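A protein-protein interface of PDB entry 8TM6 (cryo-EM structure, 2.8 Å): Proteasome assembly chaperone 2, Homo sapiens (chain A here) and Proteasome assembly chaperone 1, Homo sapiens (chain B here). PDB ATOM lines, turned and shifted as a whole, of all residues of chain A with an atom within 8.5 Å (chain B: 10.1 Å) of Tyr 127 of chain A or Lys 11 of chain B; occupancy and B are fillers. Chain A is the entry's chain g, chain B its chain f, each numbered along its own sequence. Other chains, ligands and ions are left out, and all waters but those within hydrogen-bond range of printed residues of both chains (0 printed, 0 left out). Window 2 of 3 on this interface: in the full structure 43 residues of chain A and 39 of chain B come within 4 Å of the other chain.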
ATOM      1  N   VAL A  24     -17.828 -21.383   4.827  1.00  0.00           N
ATOM      2  CA  VAL A  24     -17.838 -22.398   3.777  1.00  0.00           C
ATOM      3  C   VAL A  24     -17.156 -21.863   2.524  1.00  0.00           C
ATOM      4  O   VAL A  24     -16.325 -22.541   1.909  1.00  0.00           O
ATOM      5  CB  VAL A  24     -19.279 -22.849   3.482  1.00  0.00           C
ATOM      6  CG1 VAL A  24     -19.299 -23.886   2.368  1.00  0.00           C
ATOM      7  CG2 VAL A  24     -19.932 -23.400   4.741  1.00  0.00           C
ATOM      8  N   SER A 124     -22.789 -20.992   7.087  1.00  0.00           N
ATOM      9  CA  SER A 124     -23.022 -22.414   7.279  1.00  0.00           C
ATOM     10  C   SER A 124     -23.385 -23.060   5.947  1.00  0.00           C
ATOM     11  O   SER A 124     -23.704 -22.385   4.965  1.00  0.00           O
ATOM     12  CB  SER A 124     -24.133 -22.655   8.308  1.00  0.00           C
ATOM     13  OG  SER A 124     -24.164 -24.010   8.715  1.00  0.00           O
ATOM     14  N   HIS A 125     -23.332 -24.388   5.927  1.00  0.00           N
ATOM     15  CA  HIS A 125     -23.627 -25.139   4.716  1.00  0.00           C
ATOM     16  C   HIS A 125     -25.111 -25.041   4.391  1.00  0.00           C
ATOM     17  O   HIS A 125     -25.964 -25.274   5.253  1.00  0.00           O
ATOM     18  CB  HIS A 125     -23.219 -26.601   4.887  1.00  0.00           C
ATOM     19  CG  HIS A 125     -21.765 -26.855   4.636  1.00  0.00           C
ATOM     20  ND1 HIS A 125     -20.947 -27.466   5.560  1.00  0.00           N
ATOM     21  CD2 HIS A 125     -20.986 -26.580   3.564  1.00  0.00           C
ATOM     22  CE1 HIS A 125     -19.723 -27.555   5.070  1.00  0.00           C
ATOM     23  NE2 HIS A 125     -19.720 -27.025   3.861  1.00  0.00           N
ATOM     24  N   SER A 126     -25.417 -24.698   3.140  1.00  0.00           N
ATOM     25  CA  SER A 126     -26.800 -24.572   2.704  1.00  0.00           C
ATOM     26  C   SER A 126     -27.451 -25.912   2.400  1.00  0.00           C
ATOM     27  O   SER A 126     -28.674 -25.960   2.227  1.00  0.00           O
ATOM     28  CB  SER A 126     -26.879 -23.676   1.465  1.00  0.00           C
ATOM     29  OG  SER A 126     -28.193 -23.656   0.934  1.00  0.00           O
ATOM     30  N   TYR A 127     -26.676 -26.994   2.332  1.00  0.00           N
ATOM     31  CA  TYR A 127     -27.217 -28.304   1.993  1.00  0.00           C
ATOM     32  C   TYR A 127     -27.332 -29.236   3.192  1.00  0.00           C
ATOM     33  O   TYR A 127     -28.067 -30.225   3.118  1.00  0.00           O
ATOM     34  CB  TYR A 127     -26.363 -28.952   0.895  1.00  0.00           C
ATOM     35  CG  TYR A 127     -25.018 -29.470   1.340  1.00  0.00           C
ATOM     36  CD1 TYR A 127     -24.879 -30.751   1.851  1.00  0.00           C
ATOM     37  CD2 TYR A 127     -23.883 -28.680   1.238  1.00  0.00           C
ATOM     38  CE1 TYR A 127     -23.651 -31.230   2.248  1.00  0.00           C
ATOM     39  CE2 TYR A 127     -22.649 -29.149   1.635  1.00  0.00           C
ATOM     40  CZ  TYR A 127     -22.539 -30.424   2.139  1.00  0.00           C
ATOM     41  OH  TYR A 127     -21.311 -30.897   2.539  1.00  0.00           O
ATOM     42  N   GLN A 128     -26.630 -28.954   4.290  1.00  0.00           N
ATOM     43  CA  GLN A 128     -26.945 -29.573   5.579  1.00  0.00           C
ATOM     44  C   GLN A 128     -28.006 -28.741   6.302  1.00  0.00           C
ATOM     45  O   GLN A 128     -27.850 -28.332   7.451  1.00  0.00           O
ATOM     46  CB  GLN A 128     -25.691 -29.721   6.438  1.00  0.00           C
ATOM     47  CG  GLN A 128     -24.766 -30.870   6.059  1.00  0.00           C
ATOM     48  CD  GLN A 128     -23.299 -30.524   6.247  1.00  0.00           C
ATOM     49  OE1 GLN A 128     -22.899 -30.033   7.300  1.00  0.00           O
ATOM     50  NE2 GLN A 128     -22.487 -30.809   5.240  1.00  0.00           N
ATOM     51  N   ARG A 129     -29.108 -28.498   5.595  1.00  0.00           N
ATOM     52  CA  ARG A 129     -30.140 -27.574   6.045  1.00  0.00           C
ATOM     53  C   ARG A 129     -31.452 -28.323   6.215  1.00  0.00           C
ATOM     54  O   ARG A 129     -31.807 -29.162   5.382  1.00  0.00           O
ATOM     55  CB  ARG A 129     -30.308 -26.421   5.052  1.00  0.00           C
ATOM     56  CG  ARG A 129     -31.296 -25.357   5.493  1.00  0.00           C
ATOM     57  CD  ARG A 129     -31.148 -24.074   4.685  1.00  0.00           C
ATOM     58  NE  ARG A 129     -30.897 -24.319   3.269  1.00  0.00           N
ATOM     59  CZ  ARG A 129     -31.061 -23.417   2.311  1.00  0.00           C
ATOM     60  NH1 ARG A 129     -31.479 -22.191   2.580  1.00  0.00           N
ATOM     61  NH2 ARG A 129     -30.800 -23.753   1.051  1.00  0.00           N
ATOM     62  N   ASN A 130     -32.166 -28.013   7.294  1.00  0.00           N
ATOM     63  CA  ASN A 130     -33.418 -28.678   7.611  1.00  0.00           C
ATOM     64  C   ASN A 130     -34.557 -28.112   6.764  1.00  0.00           C
ATOM     65  O   ASN A 130     -34.442 -27.058   6.134  1.00  0.00           O
ATOM     66  CB  ASN A 130     -33.733 -28.525   9.099  1.00  0.00           C
ATOM     67  CG  ASN A 130     -34.835 -29.454   9.560  1.00  0.00           C
ATOM     68  OD1 ASN A 130     -35.445 -30.158   8.757  1.00  0.00           O
ATOM     69  ND2 ASN A 130     -35.102 -29.456  10.861  1.00  0.00           N
ATOM     70  N   GLN A 133     -35.629 -24.718   8.129  1.00  0.00           N
ATOM     71  CA  GLN A 133     -34.621 -23.742   7.730  1.00  0.00           C
ATOM     72  C   GLN A 133     -34.609 -23.549   6.220  1.00  0.00           C
ATOM     73  O   GLN A 133     -34.347 -22.440   5.740  1.00  0.00           O
ATOM     74  CB  GLN A 133     -33.237 -24.177   8.215  1.00  0.00           C
ATOM     75  CG  GLN A 133     -33.168 -24.561   9.685  1.00  0.00           C
ATOM     76  CD  GLN A 133     -31.904 -25.324  10.027  1.00  0.00           C
ATOM     77  OE1 GLN A 133     -31.150 -25.728   9.142  1.00  0.00           O
ATOM     78  NE2 GLN A 133     -31.665 -25.526  11.317  1.00  0.00           N
ATOM     79  N   LEU A 134     -34.885 -24.611   5.462  1.00  0.00           N
ATOM     80  CA  LEU A 134     -34.925 -24.489   4.009  1.00  0.00           C
ATOM     81  C   LEU A 134     -36.022 -23.530   3.570  1.00  0.00           C
ATOM     82  O   LEU A 134     -35.814 -22.709   2.668  1.00  0.00           O
ATOM     83  CB  LEU A 134     -35.131 -25.868   3.378  1.00  0.00           C
ATOM     84  CG  LEU A 134     -34.962 -26.010   1.863  1.00  0.00           C
ATOM     85  CD1 LEU A 134     -33.879 -25.091   1.316  1.00  0.00           C
ATOM     86  CD2 LEU A 134     -34.654 -27.456   1.516  1.00  0.00           C
ATOM     87  N   PRO A 182     -23.100 -26.587  10.921  1.00  0.00           N
ATOM     88  CA  PRO A 182     -22.504 -27.582  10.011  1.00  0.00           C
ATOM     89  C   PRO A 182     -21.343 -27.061   9.182  1.00  0.00           C
ATOM     90  O   PRO A 182     -20.373 -27.797   8.969  1.00  0.00           O
ATOM     91  CB  PRO A 182     -23.686 -27.999   9.118  1.00  0.00           C
ATOM     92  CG  PRO A 182     -24.803 -27.061   9.419  1.00  0.00           C
ATOM     93  CD  PRO A 182     -24.561 -26.492  10.767  1.00  0.00           C
ATOM     94  N   GLY A 183     -21.412 -25.822   8.698  1.00  0.00           N
ATOM     95  CA  GLY A 183     -20.377 -25.269   7.847  1.00  0.00           C
ATOM     96  C   GLY A 183     -19.616 -24.098   8.422  1.00  0.00           C
ATOM     97  O   GLY A 183     -18.848 -23.461   7.689  1.00  0.00           O
ATOM     98  N   PHE A 207     -26.819 -19.471   5.585  1.00  0.00           N
ATOM     99  CA  PHE A 207     -26.749 -20.734   4.858  1.00  0.00           C
ATOM    100  C   PHE A 207     -26.387 -20.456   3.405  1.00  0.00           C
ATOM    101  O   PHE A 207     -27.199 -19.914   2.647  1.00  0.00           O
ATOM    102  CB  PHE A 207     -28.078 -21.477   4.961  1.00  0.00           C
ATOM    103  CG  PHE A 207     -28.438 -21.884   6.361  1.00  0.00           C
ATOM    104  CD1 PHE A 207     -27.611 -22.725   7.086  1.00  0.00           C
ATOM    105  CD2 PHE A 207     -29.601 -21.426   6.953  1.00  0.00           C
ATOM    106  CE1 PHE A 207     -27.939 -23.101   8.373  1.00  0.00           C
ATOM    107  CE2 PHE A 207     -29.934 -21.799   8.240  1.00  0.00           C
ATOM    108  CZ  PHE A 207     -29.101 -22.637   8.950  1.00  0.00           C
ATOM    109  N   VAL A 208     -25.169 -20.827   3.012  1.00  0.00           N
ATOM    110  CA  VAL A 208     -24.644 -20.541   1.685  1.00  0.00           C
ATOM    111  C   VAL A 208     -24.053 -21.818   1.101  1.00  0.00           C
ATOM    112  O   VAL A 208     -23.875 -22.824   1.788  1.00  0.00           O
ATOM    113  CB  VAL A 208     -23.582 -19.422   1.706  1.00  0.00           C
ATOM    114  CG1 VAL A 208     -24.025 -18.283   2.609  1.00  0.00           C
ATOM    115  CG2 VAL A 208     -22.236 -19.973   2.158  1.00  0.00           C
ATOM    116  N   SER A 209     -23.752 -21.758  -0.190  1.00  0.00           N
ATOM    117  CA  SER A 209     -23.067 -22.819  -0.911  1.00  0.00           C
ATOM    118  C   SER A 209     -21.738 -22.272  -1.431  1.00  0.00           C
ATOM    119  O   SER A 209     -21.349 -21.140  -1.131  1.00  0.00           O
ATOM    120  CB  SER A 209     -23.948 -23.356  -2.042  1.00  0.00           C
ATOM    121  OG  SER A 209     -25.102 -23.996  -1.529  1.00  0.00           O
ATOM    122  N   GLU A 210     -21.041 -23.083  -2.220  1.00  0.00           N
ATOM    123  CA  GLU A 210     -19.740 -22.716  -2.757  1.00  0.00           C
ATOM    124  C   GLU A 210     -19.879 -22.212  -4.187  1.00  0.00           C
ATOM    125  O   GLU A 210     -20.621 -22.784  -4.990  1.00  0.00           O
ATOM    126  CB  GLU A 210     -18.780 -23.904  -2.716  1.00  0.00           C
ATOM    127  CG  GLU A 210     -17.936 -23.974  -1.452  1.00  0.00           C
ATOM    128  CD  GLU A 210     -16.541 -23.401  -1.633  1.00  0.00           C
ATOM    129  OE1 GLU A 210     -16.061 -23.330  -2.784  1.00  0.00           O
ATOM    130  OE2 GLU A 210     -15.922 -23.021  -0.618  1.00  0.00           O
ATOM    131  N   MET B   1     -16.942 -36.288  -3.011  1.00  0.00           N
ATOM    132  CA  MET B   1     -16.393 -36.231  -4.395  1.00  0.00           C
ATOM    133  C   MET B   1     -15.792 -37.575  -4.792  1.00  0.00           C
ATOM    134  O   MET B   1     -14.744 -37.632  -5.433  1.00  0.00           O
ATOM    135  CB  MET B   1     -15.337 -35.130  -4.508  1.00  0.00           C
ATOM    136  N   ALA B   2     -16.467 -38.657  -4.406  1.00  0.00           N
ATOM    137  CA  ALA B   2     -16.001 -40.005  -4.718  1.00  0.00           C
ATOM    138  C   ALA B   2     -16.624 -40.521  -6.013  1.00  0.00           C
ATOM    139  O   ALA B   2     -15.911 -40.834  -6.972  1.00  0.00           O
ATOM    140  CB  ALA B   2     -16.319 -40.950  -3.554  1.00  0.00           C
ATOM    141  N   ALA B   3     -17.953 -40.608  -6.054  1.00  0.00           N
ATOM    142  CA  ALA B   3     -18.668 -41.077  -7.238  1.00  0.00           C
ATOM    143  C   ALA B   3     -18.167 -42.450  -7.674  1.00  0.00           C
ATOM    144  O   ALA B   3     -18.042 -42.743  -8.866  1.00  0.00           O
ATOM    145  CB  ALA B   3     -18.548 -40.067  -8.381  1.00  0.00           C
ATOM    146  N   THR B   4     -17.875 -43.308  -6.694  1.00  0.00           N
ATOM    147  CA  THR B   4     -17.401 -44.652  -7.011  1.00  0.00           C
ATOM    148  C   THR B   4     -18.473 -45.459  -7.731  1.00  0.00           C
ATOM    149  O   THR B   4     -18.174 -46.184  -8.687  1.00  0.00           O
ATOM    150  CB  THR B   4     -16.959 -45.374  -5.739  1.00  0.00           C
ATOM    151  OG1 THR B   4     -18.039 -45.395  -4.798  1.00  0.00           O
ATOM    152  CG2 THR B   4     -15.761 -44.677  -5.118  1.00  0.00           C
ATOM    153  N   GLY B   7     -25.136 -44.421  -7.152  1.00  0.00           N
ATOM    154  CA  GLY B   7     -25.874 -43.629  -6.188  1.00  0.00           C
ATOM    155  C   GLY B   7     -25.019 -43.002  -5.108  1.00  0.00           C
ATOM    156  O   GLY B   7     -25.549 -42.494  -4.115  1.00  0.00           O
ATOM    157  N   GLU B   8     -23.702 -43.024  -5.284  1.00  0.00           N
ATOM    158  CA  GLU B   8     -22.804 -42.475  -4.278  1.00  0.00           C
ATOM    159  C   GLU B   8     -23.111 -40.997  -4.072  1.00  0.00           C
ATOM    160  O   GLU B   8     -23.234 -40.240  -5.041  1.00  0.00           O
ATOM    161  CB  GLU B   8     -21.350 -42.677  -4.702  1.00  0.00           C
ATOM    162  CG  GLU B   8     -20.321 -41.966  -3.829  1.00  0.00           C
ATOM    163  CD  GLU B   8     -20.156 -42.611  -2.467  1.00  0.00           C
ATOM    164  OE1 GLU B   8     -21.090 -43.305  -2.013  1.00  0.00           O
ATOM    165  OE2 GLU B   8     -19.091 -42.418  -1.845  1.00  0.00           O
ATOM    166  N   VAL B   9     -23.235 -40.587  -2.813  1.00  0.00           N
ATOM    167  CA  VAL B   9     -23.513 -39.195  -2.480  1.00  0.00           C
ATOM    168  C   VAL B   9     -22.183 -38.452  -2.425  1.00  0.00           C
ATOM    169  O   VAL B   9     -21.340 -38.728  -1.568  1.00  0.00           O
ATOM    170  CB  VAL B   9     -24.275 -39.072  -1.155  1.00  0.00           C
ATOM    171  CG1 VAL B   9     -24.408 -37.611  -0.751  1.00  0.00           C
ATOM    172  CG2 VAL B   9     -25.642 -39.724  -1.270  1.00  0.00           C
ATOM    173  N   VAL B  10     -21.993 -37.509  -3.339  1.00  0.00           N
ATOM    174  CA  VAL B  10     -20.775 -36.715  -3.407  1.00  0.00           C
ATOM    175  C   VAL B  10     -21.030 -35.377  -2.732  1.00  0.00           C
ATOM    176  O   VAL B  10     -22.153 -34.859  -2.728  1.00  0.00           O
ATOM    177  CB  VAL B  10     -20.304 -36.524  -4.865  1.00  0.00           C
ATOM    178  CG1 VAL B  10     -20.054 -37.873  -5.521  1.00  0.00           C
ATOM    179  CG2 VAL B  10     -21.320 -35.717  -5.664  1.00  0.00           C
ATOM    180  N   LYS B  11     -19.975 -34.809  -2.154  1.00  0.00           N
ATOM    181  CA  LYS B  11     -20.043 -33.530  -1.466  1.00  0.00           C
ATOM    182  C   LYS B  11     -19.098 -32.544  -2.134  1.00  0.00           C
ATOM    183  O   LYS B  11     -17.971 -32.896  -2.496  1.00  0.00           O
ATOM    184  CB  LYS B  11     -19.682 -33.677   0.015  1.00  0.00           C
ATOM    185  CG  LYS B  11     -20.846 -34.108   0.893  1.00  0.00           C
ATOM    186  CD  LYS B  11     -20.407 -34.976   2.073  1.00  0.00           C
ATOM    187  CE  LYS B  11     -19.246 -34.374   2.864  1.00  0.00           C
ATOM    188  NZ  LYS B  11     -18.592 -35.391   3.732  1.00  0.00           N
ATOM    189  N   ALA B  12     -19.562 -31.315  -2.293  1.00  0.00           N
ATOM    190  CA  ALA B  12     -18.750 -30.284  -2.919  1.00  0.00           C
ATOM    191  C   ALA B  12     -17.587 -29.919  -2.005  1.00  0.00           C
ATOM    192  O   ALA B  12     -17.821 -29.538  -0.850  1.00  0.00           O
ATOM    193  CB  ALA B  12     -19.601 -29.053  -3.212  1.00  0.00           C
ATOM    194  N   PRO B  13     -16.337 -30.019  -2.456  1.00  0.00           N
ATOM    195  CA  PRO B  13     -15.221 -29.625  -1.590  1.00  0.00           C
ATOM    196  C   PRO B  13     -15.268 -28.138  -1.278  1.00  0.00           C
ATOM    197  O   PRO B  13     -15.686 -27.323  -2.105  1.00  0.00           O
ATOM    198  CB  PRO B  13     -13.981 -29.992  -2.412  1.00  0.00           C
ATOM    199  CG  PRO B  13     -14.445 -29.994  -3.822  1.00  0.00           C
ATOM    200  CD  PRO B  13     -15.875 -30.440  -3.790  1.00  0.00           C
ATOM    201  N   CYS B  14     -14.833 -27.789  -0.071  1.00  0.00           N
ATOM    202  CA  CYS B  14     -14.808 -26.402   0.370  1.00  0.00           C
ATOM    203  C   CYS B  14     -13.412 -25.828   0.169  1.00  0.00           C
ATOM    204  O   CYS B  14     -12.424 -26.404   0.636  1.00  0.00           O
ATOM    205  CB  CYS B  14     -15.216 -26.295   1.839  1.00  0.00           C
ATOM    206  SG  CYS B  14     -16.734 -27.181   2.256  1.00  0.00           S
ATOM    207  N   ARG B  15     -13.334 -24.692  -0.529  1.00  0.00           N
ATOM    208  CA  ARG B  15     -12.047 -24.042  -0.732  1.00  0.00           C
ATOM    209  C   ARG B  15     -11.435 -23.568   0.577  1.00  0.00           C
ATOM    210  O   ARG B  15     -10.224 -23.331   0.632  1.00  0.00           O
ATOM    211  CB  ARG B  15     -12.196 -22.866  -1.699  1.00  0.00           C
ATOM    212  CG  ARG B  15     -12.882 -21.641  -1.121  1.00  0.00           C
ATOM    213  CD  ARG B  15     -12.976 -20.537  -2.159  1.00  0.00           C
ATOM    214  NE  ARG B  15     -14.037 -20.787  -3.128  1.00  0.00           N
ATOM    215  CZ  ARG B  15     -15.207 -20.161  -3.154  1.00  0.00           C
ATOM    216  NH1 ARG B  15     -15.524 -19.240  -2.257  1.00  0.00           N
ATOM    217  NH2 ARG B  15     -16.086 -20.468  -4.103  1.00  0.00           N
ATOM    218  N   THR B  18     -12.915 -26.498   5.263  1.00  0.00           N
ATOM    219  CA  THR B  18     -13.670 -26.720   6.490  1.00  0.00           C
ATOM    220  C   THR B  18     -13.905 -28.205   6.731  1.00  0.00           C
ATOM    221  O   THR B  18     -13.783 -28.682   7.865  1.00  0.00           O
ATOM    222  CB  THR B  18     -15.000 -25.969   6.429  1.00  0.00           C
ATOM    223  OG1 THR B  18     -14.758 -24.557   6.489  1.00  0.00           O
ATOM    224  CG2 THR B  18     -15.901 -26.373   7.585  1.00  0.00           C
ATOM    225  N   GLU B  19     -14.223 -28.958   5.674  1.00  0.00           N
ATOM    226  CA  GLU B  19     -14.599 -30.359   5.842  1.00  0.00           C
ATOM    227  C   GLU B  19     -13.524 -31.153   6.572  1.00  0.00           C
ATOM    228  O   GLU B  19     -13.843 -32.061   7.351  1.00  0.00           O
ATOM    229  CB  GLU B  19     -14.883 -30.989   4.477  1.00  0.00           C
ATOM    230  CG  GLU B  19     -15.831 -30.172   3.605  1.00  0.00           C
ATOM    231  CD  GLU B  19     -16.765 -31.032   2.774  1.00  0.00           C
ATOM    232  OE1 GLU B  19     -17.728 -30.481   2.202  1.00  0.00           O
ATOM    233  OE2 GLU B  19     -16.538 -32.257   2.686  1.00  0.00           O
ATOM    234  N   ASP B  20     -12.250 -30.833   6.338  1.00  0.00           N
ATOM    235  CA  ASP B  20     -11.175 -31.530   7.038  1.00  0.00           C
ATOM    236  C   ASP B  20     -11.318 -31.367   8.546  1.00  0.00           C
ATOM    237  O   ASP B  20     -11.273 -32.347   9.298  1.00  0.00           O
ATOM    238  CB  ASP B  20      -9.819 -31.008   6.564  1.00  0.00           C
ATOM    239  CG  ASP B  20      -9.601 -31.216   5.077  1.00  0.00           C
ATOM    240  OD1 ASP B  20     -10.337 -32.025   4.475  1.00  0.00           O
ATOM    241  OD2 ASP B  20      -8.694 -30.570   4.514  1.00  0.00           O
ATOM    242  N   GLU B  22     -14.061 -30.441  10.135  1.00  0.00           N
ATOM    243  CA  GLU B  22     -15.341 -30.995  10.563  1.00  0.00           C
ATOM    244  C   GLU B  22     -15.221 -32.486  10.837  1.00  0.00           C
ATOM    245  O   GLU B  22     -15.735 -32.984  11.845  1.00  0.00           O
ATOM    246  CB  GLU B  22     -16.416 -30.725   9.508  1.00  0.00           C
ATOM    247  CG  GLU B  22     -16.575 -29.257   9.145  1.00  0.00           C
ATOM    248  CD  GLU B  22     -17.410 -28.493  10.152  1.00  0.00           C
ATOM    249  OE1 GLU B  22     -17.445 -28.902  11.331  1.00  0.00           O
ATOM    250  OE2 GLU B  22     -18.016 -27.472   9.769  1.00  0.00           O
ATOM    251  N   GLU B  23     -14.546 -33.218   9.950  1.00  0.00           N
ATOM    252  CA  GLU B  23     -14.240 -34.613  10.248  1.00  0.00           C
ATOM    253  C   GLU B  23     -13.335 -34.728  11.468  1.00  0.00           C
ATOM    254  O   GLU B  23     -13.578 -35.559  12.351  1.00  0.00           O
ATOM    255  CB  GLU B  23     -13.589 -35.288   9.042  1.00  0.00           C
ATOM    256  CG  GLU B  23     -12.647 -36.434   9.410  1.00  0.00           C
ATOM    257  CD  GLU B  23     -13.337 -37.552  10.182  1.00  0.00           C
ATOM    258  OE1 GLU B  23     -14.529 -37.402  10.525  1.00  0.00           O
ATOM    259  OE2 GLU B  23     -12.677 -38.573  10.466  1.00  0.00           O
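The guanidinium group (NH2) of Arg 15 of chain B is in salt-bridge range of the side-chain carboxylate (OE1) of Glu 210 of chain A, at 3.2 Å. SG of Cys 14 of chain B sits at hydrogen-bond distance from NE2 of His 125 of chain A (3.4 Å). The side-chain carboxylate (OE2) of Glu 22 of chain B lies close to the backbone carbonyl oxygen (O) of Pro 182 of chain A (2.5 Å).
The backbone carbonyl oxygen (O) of Val 24 of chain A sits close to the side-chain carboxylate (OE2) of Glu 210 of chain A (2.6 Å). The side-chain hydroxyl of Tyr 127 of chain A lies within hydrogen-bond range of the side-chain amide nitrogen of Gln 128 of chain A (2.9 Å). The side-chain sulfur (SG) of Cys 14 of chain B lies close to the side-chain carboxylate (OE1) of Glu 19 of chain B (3.4 Å). ND1 of His 125 of chain A sits at hydrogen-bond distance from O of Pro 182 of chain A, at 3.5 Å. NZ of Lys 11 of chain B lies within salt-bridge range of OE2 of Glu 19 of chain B (3.9 Å). The side-chain hydroxyl (OG) of Ser 124 of chain A lies within hydrogen-bond range of the backbone NH (N) of Gly 183 of chain A, 3.3 Å away.
CB of Cys 14 of chain B touches O of Val 24 of chain A, 3.9 Å away. OH of Tyr 127 of chain A touches CG of Lys 11 of chain B (3.6 Å). Tyr 127 of chain A touches Glu 19 of chain B (OH to OE1, 3.6 Å). Gly 183 of chain A touches Glu 22 of chain B. CA of Cys 14 of chain B touches OE2 of Glu 210 of chain A, at 3.7 Å.
Of the printed residues of chain B, Val 24 of chain A touches Cys 14. No residue of chain B comes within 4 Å of Ser 126 of chain A. Tyr 127 of chain A touches just these residues of chain B: Lys 11 (3.6 Å) and Glu 19 (3.6 Å). No residue of chain B comes within 4 Å of Gln 128 of chain A. Printed residues of chain B within 4 Å of Glu 210 of chain A: Cys 14 and Arg 15. Of the printed residues of chain A, Arg 15 of chain B touches Glu 210 (3.1 Å). Of the printed residues of chain A, Glu 19 of chain B touches Tyr 127 (3.6 Å). Of the printed residues of chain A, Glu 22 of chain B touches Pro 182 and Gly 183. Glu 23 of chain B touches none of the printed residues of chain A. The nearest residue of chain B that does not touch Tyr 127 of chain A is Ala 12 of chain B (5.1 Å). The nearest printed residue of chain A that does not touch Glu 22 of chain B is His 125 of chain A (5.0 Å).
Among the printed residues, Asp or Glu carboxylates within 4 Å of a Lys or Arg side-chain nitrogen of the other chain: Glu 210 of chain A with Arg 15 of chain B.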
